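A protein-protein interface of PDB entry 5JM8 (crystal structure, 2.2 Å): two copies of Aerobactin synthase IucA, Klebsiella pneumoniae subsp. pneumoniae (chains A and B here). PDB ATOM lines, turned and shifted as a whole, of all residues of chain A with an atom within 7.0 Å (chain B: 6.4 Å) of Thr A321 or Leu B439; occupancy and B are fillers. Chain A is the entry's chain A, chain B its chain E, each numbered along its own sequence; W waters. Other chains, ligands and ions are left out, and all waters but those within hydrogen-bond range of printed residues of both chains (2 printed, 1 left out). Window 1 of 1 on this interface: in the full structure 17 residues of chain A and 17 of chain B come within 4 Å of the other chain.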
ATOM      1  N   GLN A 316      27.598  10.500   7.586  1.00  0.00           N
ATOM      2  CA  GLN A 316      28.260  11.630   6.940  1.00  0.00           C
ATOM      3  C   GLN A 316      27.820  11.763   5.488  1.00  0.00           C
ATOM      4  O   GLN A 316      27.717  12.870   4.959  1.00  0.00           O
ATOM      5  CB  GLN A 316      29.783  11.475   7.011  1.00  0.00           C
ATOM      6  CG  GLN A 316      30.564  12.634   6.395  1.00  0.00           C
ATOM      7  CD  GLN A 316      30.323  13.955   7.106  1.00  0.00           C
ATOM      8  OE1 GLN A 316      30.987  14.271   8.092  1.00  0.00           O
ATOM      9  NE2 GLN A 316      29.377  14.738   6.600  1.00  0.00           N
ATOM     10  N   ALA A 317      27.567  10.630   4.844  1.00  0.00           N
ATOM     11  CA  ALA A 317      27.157  10.614   3.447  1.00  0.00           C
ATOM     12  C   ALA A 317      25.759  11.192   3.285  1.00  0.00           C
ATOM     13  O   ALA A 317      25.463  11.872   2.302  1.00  0.00           O
ATOM     14  CB  ALA A 317      27.204   9.199   2.901  1.00  0.00           C
ATOM     15  N   ARG A 318      24.904  10.915   4.264  1.00  0.00           N
ATOM     16  CA  ARG A 318      23.514  11.357   4.236  1.00  0.00           C
ATOM     17  C   ARG A 318      23.410  12.858   4.475  1.00  0.00           C
ATOM     18  O   ARG A 318      22.487  13.514   3.989  1.00  0.00           O
ATOM     19  CB  ARG A 318      22.710  10.593   5.287  1.00  0.00           C
ATOM     20  CG  ARG A 318      21.236  10.940   5.342  1.00  0.00           C
ATOM     21  CD  ARG A 318      20.543  10.106   6.404  1.00  0.00           C
ATOM     22  NE  ARG A 318      19.135  10.456   6.578  1.00  0.00           N
ATOM     23  CZ  ARG A 318      18.319   9.851   7.435  1.00  0.00           C
ATOM     24  NH1 ARG A 318      18.769   8.863   8.201  1.00  0.00           N
ATOM     25  NH2 ARG A 318      17.053  10.232   7.532  1.00  0.00           N
ATOM     26  N   PHE A 319      24.365  13.386   5.237  1.00  0.00           N
ATOM     27  CA  PHE A 319      24.457  14.818   5.503  1.00  0.00           C
ATOM     28  C   PHE A 319      25.866  15.314   5.181  1.00  0.00           C
ATOM     29  O   PHE A 319      26.692  15.472   6.080  1.00  0.00           O
ATOM     30  CB  PHE A 319      24.114  15.123   6.962  1.00  0.00           C
ATOM     31  CG  PHE A 319      22.745  14.664   7.371  1.00  0.00           C
ATOM     32  CD1 PHE A 319      21.633  15.446   7.114  1.00  0.00           C
ATOM     33  CD2 PHE A 319      22.571  13.453   8.020  1.00  0.00           C
ATOM     34  CE1 PHE A 319      20.371  15.026   7.492  1.00  0.00           C
ATOM     35  CE2 PHE A 319      21.314  13.030   8.401  1.00  0.00           C
ATOM     36  CZ  PHE A 319      20.212  13.818   8.137  1.00  0.00           C
ATOM     37  N   PRO A 320      26.151  15.551   3.892  1.00  0.00           N
ATOM     38  CA  PRO A 320      27.499  15.958   3.481  1.00  0.00           C
ATOM     39  C   PRO A 320      27.915  17.340   3.990  1.00  0.00           C
ATOM     40  O   PRO A 320      29.112  17.608   4.117  1.00  0.00           O
ATOM     41  CB  PRO A 320      27.410  15.954   1.952  1.00  0.00           C
ATOM     42  CG  PRO A 320      25.968  16.183   1.656  1.00  0.00           C
ATOM     43  CD  PRO A 320      25.228  15.468   2.746  1.00  0.00           C
ATOM     44  N   THR A 321      26.944  18.202   4.273  1.00  0.00           N
ATOM     45  CA  THR A 321      27.233  19.559   4.724  1.00  0.00           C
ATOM     46  C   THR A 321      27.404  19.634   6.239  1.00  0.00           C
ATOM     47  O   THR A 321      27.741  20.690   6.780  1.00  0.00           O
ATOM     48  CB  THR A 321      26.124  20.530   4.315  1.00  0.00           C
ATOM     49  OG1 THR A 321      24.884  20.112   4.896  1.00  0.00           O
ATOM     50  CG2 THR A 321      25.986  20.577   2.803  1.00  0.00           C
ATOM     51  N   PHE A 322      27.169  18.512   6.916  1.00  0.00           N
ATOM     52  CA  PHE A 322      27.338  18.431   8.363  1.00  0.00           C
ATOM     53  C   PHE A 322      28.713  17.874   8.719  1.00  0.00           C
ATOM     54  O   PHE A 322      29.091  16.800   8.253  1.00  0.00           O
ATOM     55  CB  PHE A 322      26.240  17.560   8.979  1.00  0.00           C
ATOM     56  CG  PHE A 322      26.507  17.167  10.406  1.00  0.00           C
ATOM     57  CD1 PHE A 322      26.672  18.131  11.384  1.00  0.00           C
ATOM     58  CD2 PHE A 322      26.586  15.832  10.769  1.00  0.00           C
ATOM     59  CE1 PHE A 322      26.917  17.775  12.698  1.00  0.00           C
ATOM     60  CE2 PHE A 322      26.830  15.470  12.082  1.00  0.00           C
ATOM     61  CZ  PHE A 322      26.994  16.444  13.047  1.00  0.00           C
ATOM     62  N   ARG A 323      29.458  18.616   9.538  1.00  0.00           N
ATOM     63  CA  ARG A 323      30.748  18.148  10.043  1.00  0.00           C
ATOM     64  C   ARG A 323      30.791  18.189  11.564  1.00  0.00           C
ATOM     65  O   ARG A 323      30.110  18.994  12.195  1.00  0.00           O
ATOM     66  CB  ARG A 323      31.903  18.995   9.493  1.00  0.00           C
ATOM     67  CG  ARG A 323      32.049  19.006   7.979  1.00  0.00           C
ATOM     68  CD  ARG A 323      32.266  17.619   7.387  1.00  0.00           C
ATOM     69  NE  ARG A 323      33.508  16.982   7.825  1.00  0.00           N
ATOM     70  CZ  ARG A 323      34.701  17.192   7.272  1.00  0.00           C
ATOM     71  NH1 ARG A 323      34.835  18.042   6.266  1.00  0.00           N
ATOM     72  NH2 ARG A 323      35.769  16.557   7.732  1.00  0.00           N
ATOM     73  N   HIS A 407      16.983  22.964   8.240  1.00  0.00           N
ATOM     74  CA  HIS A 407      17.449  21.904   7.352  1.00  0.00           C
ATOM     75  C   HIS A 407      18.935  21.596   7.525  1.00  0.00           C
ATOM     76  O   HIS A 407      19.346  20.439   7.429  1.00  0.00           O
ATOM     77  CB  HIS A 407      17.186  22.278   5.892  1.00  0.00           C
ATOM     78  CG  HIS A 407      15.746  22.191   5.491  1.00  0.00           C
ATOM     79  ND1 HIS A 407      15.027  23.285   5.061  1.00  0.00           N
ATOM     80  CD2 HIS A 407      14.895  21.137   5.441  1.00  0.00           C
ATOM     81  CE1 HIS A 407      13.794  22.911   4.767  1.00  0.00           C
ATOM     82  NE2 HIS A 407      13.688  21.613   4.990  1.00  0.00           N
ATOM     83  N   GLN A 408      19.734  22.631   7.767  1.00  0.00           N
ATOM     84  CA  GLN A 408      21.183  22.476   7.851  1.00  0.00           C
ATOM     85  C   GLN A 408      21.685  22.152   9.255  1.00  0.00           C
ATOM     86  O   GLN A 408      22.678  21.438   9.406  1.00  0.00           O
ATOM     87  CB  GLN A 408      21.879  23.748   7.360  1.00  0.00           C
ATOM     88  CG  GLN A 408      21.663  24.053   5.884  1.00  0.00           C
ATOM     89  CD  GLN A 408      22.190  22.958   4.980  1.00  0.00           C
ATOM     90  OE1 GLN A 408      22.952  22.090   5.411  1.00  0.00           O
ATOM     91  NE2 GLN A 408      21.778  22.986   3.720  1.00  0.00           N
ATOM     92  N   PRO A 412      20.405  17.338  10.769  1.00  0.00           N
ATOM     93  CA  PRO A 412      21.442  16.341  11.059  1.00  0.00           C
ATOM     94  C   PRO A 412      21.536  15.958  12.535  1.00  0.00           C
ATOM     95  O   PRO A 412      21.880  14.820  12.847  1.00  0.00           O
ATOM     96  CB  PRO A 412      22.733  17.031  10.603  1.00  0.00           C
ATOM     97  CG  PRO A 412      22.404  18.482  10.523  1.00  0.00           C
ATOM     98  CD  PRO A 412      20.968  18.545  10.138  1.00  0.00           C
ATOM     99  N   GLN A 434      27.695  27.327   8.894  1.00  0.00           N
ATOM    100  CA  GLN A 434      28.411  27.528   7.647  1.00  0.00           C
ATOM    101  C   GLN A 434      27.509  28.250   6.662  1.00  0.00           C
ATOM    102  O   GLN A 434      26.555  27.666   6.146  1.00  0.00           O
ATOM    103  CB  GLN A 434      28.870  26.192   7.067  1.00  0.00           C
ATOM    104  CG  GLN A 434      29.764  26.318   5.840  1.00  0.00           C
ATOM    105  CD  GLN A 434      30.008  24.986   5.154  1.00  0.00           C
ATOM    106  OE1 GLN A 434      29.230  24.042   5.303  1.00  0.00           O
ATOM    107  NE2 GLN A 434      31.095  24.905   4.397  1.00  0.00           N
ATOM    108  N   VAL A 441      24.296  27.057   4.704  1.00  0.00           N
ATOM    109  CA  VAL A 441      24.458  25.996   3.715  1.00  0.00           C
ATOM    110  C   VAL A 441      25.111  24.761   4.328  1.00  0.00           C
ATOM    111  O   VAL A 441      25.386  23.784   3.630  1.00  0.00           O
ATOM    112  CB  VAL A 441      25.303  26.469   2.510  1.00  0.00           C
ATOM    113  CG1 VAL A 441      24.595  27.594   1.779  1.00  0.00           C
ATOM    114  CG2 VAL A 441      26.682  26.920   2.964  1.00  0.00           C
ATOM    115  N   GLY A 442      25.359  24.804   5.633  1.00  0.00           N
ATOM    116  CA  GLY A 442      25.961  23.677   6.319  1.00  0.00           C
ATOM    117  C   GLY A 442      26.153  23.904   7.805  1.00  0.00           C
ATOM    118  O   GLY A 442      25.920  25.002   8.311  1.00  0.00           O
ATOM    119  N   LEU A 443      26.582  22.851   8.499  1.00  0.00           N
ATOM    120  CA  LEU A 443      26.792  22.890   9.942  1.00  0.00           C
ATOM    121  C   LEU A 443      28.143  22.296  10.314  1.00  0.00           C
ATOM    122  O   LEU A 443      28.574  21.295   9.741  1.00  0.00           O
ATOM    123  CB  LEU A 443      25.674  22.132  10.670  1.00  0.00           C
ATOM    124  CG  LEU A 443      25.895  21.830  12.160  1.00  0.00           C
ATOM    125  CD1 LEU A 443      25.890  23.114  12.979  1.00  0.00           C
ATOM    126  CD2 LEU A 443      24.857  20.852  12.692  1.00  0.00           C
ATOM    127  N   ILE A 444      28.807  22.923  11.280  1.00  0.00           N
ATOM    128  CA  ILE A 444      29.988  22.339  11.899  1.00  0.00           C
ATOM    129  C   ILE A 444      29.820  22.353  13.420  1.00  0.00           C
ATOM    130  O   ILE A 444      29.725  23.416  14.036  1.00  0.00           O
ATOM    131  CB  ILE A 444      31.279  23.082  11.499  1.00  0.00           C
ATOM    132  CG1 ILE A 444      31.426  23.108   9.974  1.00  0.00           C
ATOM    133  CG2 ILE A 444      32.491  22.411  12.138  1.00  0.00           C
ATOM    134  CD1 ILE A 444      32.605  23.922   9.476  1.00  0.00           C
ATOM    135  N   GLN B 360      33.954  28.373  -5.944  1.00  0.00           N
ATOM    136  CA  GLN B 360      33.852  27.163  -6.747  1.00  0.00           C
ATOM    137  C   GLN B 360      32.489  27.110  -7.426  1.00  0.00           C
ATOM    138  O   GLN B 360      31.635  26.300  -7.071  1.00  0.00           O
ATOM    139  CB  GLN B 360      34.076  25.920  -5.881  1.00  0.00           C
ATOM    140  CG  GLN B 360      34.250  24.641  -6.682  1.00  0.00           C
ATOM    141  CD  GLN B 360      34.409  23.410  -5.811  1.00  0.00           C
ATOM    142  OE1 GLN B 360      34.209  23.460  -4.596  1.00  0.00           O
ATOM    143  NE2 GLN B 360      34.776  22.295  -6.429  1.00  0.00           N
ATOM    144  N   ALA B 382      36.519  16.331  -8.188  1.00  0.00           N
ATOM    145  CA  ALA B 382      35.753  16.978  -7.129  1.00  0.00           C
ATOM    146  C   ALA B 382      35.098  15.951  -6.205  1.00  0.00           C
ATOM    147  O   ALA B 382      35.143  16.091  -4.984  1.00  0.00           O
ATOM    148  CB  ALA B 382      34.698  17.898  -7.729  1.00  0.00           C
ATOM    149  N   LEU B 386      35.750  15.363  -2.214  1.00  0.00           N
ATOM    150  CA  LEU B 386      34.632  15.313  -1.287  1.00  0.00           C
ATOM    151  C   LEU B 386      34.674  14.041  -0.444  1.00  0.00           C
ATOM    152  O   LEU B 386      34.382  14.066   0.755  1.00  0.00           O
ATOM    153  CB  LEU B 386      33.314  15.392  -2.052  1.00  0.00           C
ATOM    154  CG  LEU B 386      32.048  15.377  -1.200  1.00  0.00           C
ATOM    155  CD1 LEU B 386      31.998  16.587  -0.277  1.00  0.00           C
ATOM    156  CD2 LEU B 386      30.831  15.334  -2.100  1.00  0.00           C
ATOM    157  N   ARG B 389      37.655  14.518   2.052  1.00  0.00           N
ATOM    158  CA  ARG B 389      37.388  15.537   3.065  1.00  0.00           C
ATOM    159  C   ARG B 389      36.414  15.049   4.139  1.00  0.00           C
ATOM    160  O   ARG B 389      36.598  15.335   5.324  1.00  0.00           O
ATOM    161  CB  ARG B 389      36.835  16.810   2.413  1.00  0.00           C
ATOM    162  CG  ARG B 389      36.577  17.941   3.408  1.00  0.00           C
ATOM    163  CD  ARG B 389      36.177  19.240   2.721  1.00  0.00           C
ATOM    164  NE  ARG B 389      34.956  19.095   1.937  1.00  0.00           N
ATOM    165  CZ  ARG B 389      33.726  19.213   2.431  1.00  0.00           C
ATOM    166  NH1 ARG B 389      33.538  19.479   3.717  1.00  0.00           N
ATOM    167  NH2 ARG B 389      32.680  19.065   1.634  1.00  0.00           N
ATOM    168  N   LEU B 390      35.388  14.312   3.723  1.00  0.00           N
ATOM    169  CA  LEU B 390      34.338  13.862   4.633  1.00  0.00           C
ATOM    170  C   LEU B 390      34.639  12.506   5.267  1.00  0.00           C
ATOM    171  O   LEU B 390      33.985  12.110   6.230  1.00  0.00           O
ATOM    172  CB  LEU B 390      33.001  13.786   3.895  1.00  0.00           C
ATOM    173  CG  LEU B 390      32.433  15.110   3.382  1.00  0.00           C
ATOM    174  CD1 LEU B 390      31.126  14.873   2.652  1.00  0.00           C
ATOM    175  CD2 LEU B 390      32.232  16.084   4.521  1.00  0.00           C
ATOM    176  N   ALA B 397      30.378   9.462  -1.874  1.00  0.00           N
ATOM    177  CA  ALA B 397      30.589  10.823  -2.347  1.00  0.00           C
ATOM    178  C   ALA B 397      29.937  11.018  -3.716  1.00  0.00           C
ATOM    179  O   ALA B 397      29.536  12.126  -4.070  1.00  0.00           O
ATOM    180  CB  ALA B 397      32.072  11.140  -2.411  1.00  0.00           C
ATOM    181  N   ALA B 400      26.075  11.396  -2.845  1.00  0.00           N
ATOM    182  CA  ALA B 400      25.776  12.680  -2.215  1.00  0.00           C
ATOM    183  C   ALA B 400      25.836  13.815  -3.226  1.00  0.00           C
ATOM    184  O   ALA B 400      24.998  14.718  -3.212  1.00  0.00           O
ATOM    185  CB  ALA B 400      26.739  12.943  -1.074  1.00  0.00           C
ATOM    186  N   TRP B 401      26.836  13.768  -4.098  1.00  0.00           N
ATOM    187  CA  TRP B 401      26.974  14.770  -5.145  1.00  0.00           C
ATOM    188  C   TRP B 401      25.734  14.743  -6.036  1.00  0.00           C
ATOM    189  O   TRP B 401      25.110  15.776  -6.285  1.00  0.00           O
ATOM    190  CB  TRP B 401      28.240  14.523  -5.970  1.00  0.00           C
ATOM    191  CG  TRP B 401      28.676  15.713  -6.777  1.00  0.00           C
ATOM    192  CD1 TRP B 401      29.709  16.559  -6.497  1.00  0.00           C
ATOM    193  CD2 TRP B 401      28.084  16.192  -7.991  1.00  0.00           C
ATOM    194  NE1 TRP B 401      29.799  17.534  -7.461  1.00  0.00           N
ATOM    195  CE2 TRP B 401      28.812  17.331  -8.389  1.00  0.00           C
ATOM    196  CE3 TRP B 401      27.009  15.770  -8.778  1.00  0.00           C
ATOM    197  CZ2 TRP B 401      28.501  18.052  -9.541  1.00  0.00           C
ATOM    198  CZ3 TRP B 401      26.703  16.487  -9.920  1.00  0.00           C
ATOM    199  CH2 TRP B 401      27.445  17.615 -10.291  1.00  0.00           C
ATOM    200  N   ALA B 404      22.623  16.038  -4.152  1.00  0.00           N
ATOM    201  CA  ALA B 404      22.653  17.492  -4.000  1.00  0.00           C
ATOM    202  C   ALA B 404      22.421  18.184  -5.337  1.00  0.00           C
ATOM    203  O   ALA B 404      21.826  19.259  -5.394  1.00  0.00           O
ATOM    204  CB  ALA B 404      23.974  17.939  -3.400  1.00  0.00           C
ATOM    205  N   VAL B 433      27.145  25.261 -11.546  1.00  0.00           N
ATOM    206  CA  VAL B 433      26.989  24.572 -10.274  1.00  0.00           C
ATOM    207  C   VAL B 433      27.769  25.313  -9.197  1.00  0.00           C
ATOM    208  O   VAL B 433      28.997  25.290  -9.185  1.00  0.00           O
ATOM    209  CB  VAL B 433      27.475  23.109 -10.351  1.00  0.00           C
ATOM    210  CG1 VAL B 433      27.206  22.378  -9.038  1.00  0.00           C
ATOM    211  CG2 VAL B 433      26.800  22.388 -11.505  1.00  0.00           C
ATOM    212  N   GLN B 434      27.049  25.983  -8.304  1.00  0.00           N
ATOM    213  CA  GLN B 434      27.671  26.625  -7.156  1.00  0.00           C
ATOM    214  C   GLN B 434      28.070  25.552  -6.156  1.00  0.00           C
ATOM    215  O   GLN B 434      27.210  24.857  -5.614  1.00  0.00           O
ATOM    216  CB  GLN B 434      26.722  27.632  -6.504  1.00  0.00           C
ATOM    217  CG  GLN B 434      27.379  28.468  -5.412  1.00  0.00           C
ATOM    218  CD  GLN B 434      26.426  29.445  -4.747  1.00  0.00           C
ATOM    219  OE1 GLN B 434      25.208  29.277  -4.792  1.00  0.00           O
ATOM    220  NE2 GLN B 434      26.984  30.469  -4.119  1.00  0.00           N
ATOM    221  N   MET B 435      29.372  25.415  -5.923  1.00  0.00           N
ATOM    222  CA  MET B 435      29.878  24.389  -5.020  1.00  0.00           C
ATOM    223  C   MET B 435      30.635  24.980  -3.840  1.00  0.00           C
ATOM    224  O   MET B 435      31.210  26.065  -3.928  1.00  0.00           O
ATOM    225  CB  MET B 435      30.788  23.416  -5.775  1.00  0.00           C
ATOM    226  CG  MET B 435      30.045  22.495  -6.725  1.00  0.00           C
ATOM    227  SD  MET B 435      31.106  21.247  -7.477  1.00  0.00           S
ATOM    228  CE  MET B 435      31.969  22.243  -8.686  1.00  0.00           C
ATOM    229  N   LEU B 436      30.614  24.245  -2.732  1.00  0.00           N
ATOM    230  CA  LEU B 436      31.370  24.596  -1.539  1.00  0.00           C
ATOM    231  C   LEU B 436      31.939  23.321  -0.932  1.00  0.00           C
ATOM    232  O   LEU B 436      31.214  22.540  -0.315  1.00  0.00           O
ATOM    233  CB  LEU B 436      30.486  25.332  -0.533  1.00  0.00           C
ATOM    234  CG  LEU B 436      31.170  25.872   0.725  1.00  0.00           C
ATOM    235  CD1 LEU B 436      32.184  26.949   0.376  1.00  0.00           C
ATOM    236  CD2 LEU B 436      30.136  26.408   1.705  1.00  0.00           C
ATOM    237  N   GLY B 437      33.237  23.111  -1.120  1.00  0.00           N
ATOM    238  CA  GLY B 437      33.873  21.873  -0.710  1.00  0.00           C
ATOM    239  C   GLY B 437      33.476  20.755  -1.653  1.00  0.00           C
ATOM    240  O   GLY B 437      33.272  19.619  -1.232  1.00  0.00           O
ATOM    241  N   ASP B 438      33.354  21.108  -2.932  1.00  0.00           N
ATOM    242  CA  ASP B 438      33.032  20.177  -4.018  1.00  0.00           C
ATOM    243  C   ASP B 438      31.606  19.620  -3.964  1.00  0.00           C
ATOM    244  O   ASP B 438      31.251  18.761  -4.776  1.00  0.00           O
ATOM    245  CB  ASP B 438      34.036  19.019  -4.034  1.00  0.00           C
ATOM    246  CG  ASP B 438      35.458  19.493  -4.240  1.00  0.00           C
ATOM    247  OD1 ASP B 438      35.691  20.275  -5.188  1.00  0.00           O
ATOM    248  OD2 ASP B 438      36.341  19.105  -3.448  1.00  0.00           O
ATOM    249  N   LEU B 439      30.796  20.114  -3.030  1.00  0.00           N
ATOM    250  CA  LEU B 439      29.386  19.737  -2.957  1.00  0.00           C
ATOM    251  C   LEU B 439      28.521  20.840  -3.557  1.00  0.00           C
ATOM    252  O   LEU B 439      28.732  22.012  -3.258  1.00  0.00           O
ATOM    253  CB  LEU B 439      28.959  19.474  -1.511  1.00  0.00           C
ATOM    254  CG  LEU B 439      27.515  18.983  -1.342  1.00  0.00           C
ATOM    255  CD1 LEU B 439      27.391  17.531  -1.779  1.00  0.00           C
ATOM    256  CD2 LEU B 439      27.022  19.155   0.085  1.00  0.00           C
ATOM    257  N   PRO B 440      27.552  20.474  -4.416  1.00  0.00           N
ATOM    258  CA  PRO B 440      26.619  21.494  -4.911  1.00  0.00           C
ATOM    259  C   PRO B 440      25.758  22.089  -3.794  1.00  0.00           C
ATOM    260  O   PRO B 440      25.093  21.346  -3.072  1.00  0.00           O
ATOM    261  CB  PRO B 440      25.755  20.723  -5.916  1.00  0.00           C
ATOM    262  CG  PRO B 440      26.574  19.543  -6.310  1.00  0.00           C
ATOM    263  CD  PRO B 440      27.354  19.177  -5.089  1.00  0.00           C
ATOM    264  N   VAL B 441      25.779  23.414  -3.663  1.00  0.00           N
ATOM    265  CA  VAL B 441      25.026  24.111  -2.623  1.00  0.00           C
ATOM    266  C   VAL B 441      24.114  25.173  -3.227  1.00  0.00           C
ATOM    267  O   VAL B 441      23.415  25.884  -2.506  1.00  0.00           O
ATOM    268  CB  VAL B 441      25.960  24.784  -1.595  1.00  0.00           C
ATOM    269  CG1 VAL B 441      26.643  23.736  -0.734  1.00  0.00           C
ATOM    270  CG2 VAL B 441      26.986  25.666  -2.295  1.00  0.00           C
ATOM    271  N   GLY B 442      24.123  25.273  -4.552  1.00  0.00           N
ATOM    272  CA  GLY B 442      23.321  26.264  -5.244  1.00  0.00           C
ATOM    273  C   GLY B 442      23.339  26.101  -6.753  1.00  0.00           C
ATOM    274  O   GLY B 442      23.993  25.203  -7.284  1.00  0.00           O
HETATM  275  O   HOH W   1      32.857  12.570   8.987  1.00  0.00           O
HETATM  276  O   HOH W   2      32.680  22.233   5.100  1.00  0.00           O
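O of Arg B389 lies within hydrogen-bond range of NH2 of Arg A323 (2.8 Å).
N of Leu A443 is in hydrogen-bond range of O of Thr A321, at 3.0 Å.
OE1 of Gln A408 lies close to O of Val A441 (3.5 Å).
The backbone carbonyl oxygen (O) of Phe A319 is in hydrogen-bond range of the side-chain amide nitrogen (NE2) of Gln A316, at 2.8 Å.
The backbone carbonyl oxygen (O) of Gly A442 sits at hydrogen-bond distance from the backbone NH (N) of Gln A434, 3.0 Å away.
NH2 of Arg B389 lies within hydrogen-bond range of O of Gly B437.
O of Leu A443 lies within hydrogen-bond range of N of Arg A323 (2.8 Å).
Among the printed residues, merely in contact across the chains: Gln A434 with Leu B436, Thr A321 with Leu B439, Arg A323 with Leu B390, Gln A316 with Leu B390, Pro A320 with Leu B390, Pro A320 with Leu B439, Val A441 with Leu B436 and Ala A317 with Ala B400.
Of the printed residues of chain B, Gln A316 touches Leu B390.
Printed residues of chain B within 4 Å of Pro A320: Leu B390 and Leu B439.
Of chain B, only Leu B439 comes within 4 Å of Thr A321.
Printed residues of chain B within 4 Å of Gln A434: Leu B436 (3.2 Å).
Leu A443 touches none of the printed residues of chain B.
Gln B434 touches none of the printed residues of chain A.
Leu B439 touches just these residues of chain A: Pro A320 and Thr A321.
The nearest residue of chain B that does not touch Thr A321 is Val B441 (4.8 Å).
The nearest residue of chain A that does not touch Leu B439 is Val A441 (6.1 Å).
Hydrophobic or aromatic side chains of chain A that line the printed part of chain B: Pro A320 and Val A441.
Along chain A the printed residues that touch a printed residue of chain B span positions 316 to 441.
Printed residues of chain B that touch a printed residue of chain A: Arg B389, Leu B390, Ala B400, Leu B436 and Leu B439.
Hydrophobic or aromatic side chains of chain B that line the printed part of chain A: Leu B390, Ala B400, Leu B436 and Leu B439.
Positions printed for both chains: 434, 441 and 442.
Of the 9 pairs that touch across the chains among the printed residues, none has its exchanged pair printed and touching as well.
Water W1 lies within hydrogen-bond range of the side-chain amide oxygen of Gln A316 (2.7 Å) and the backbone carbonyl oxygen of Leu B390 (3.0 Å).
Water W2 lies within hydrogen-bond range of NE2 of Gln A434 (3.2 Å) and NH1 of Arg B389 (3.2 Å).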
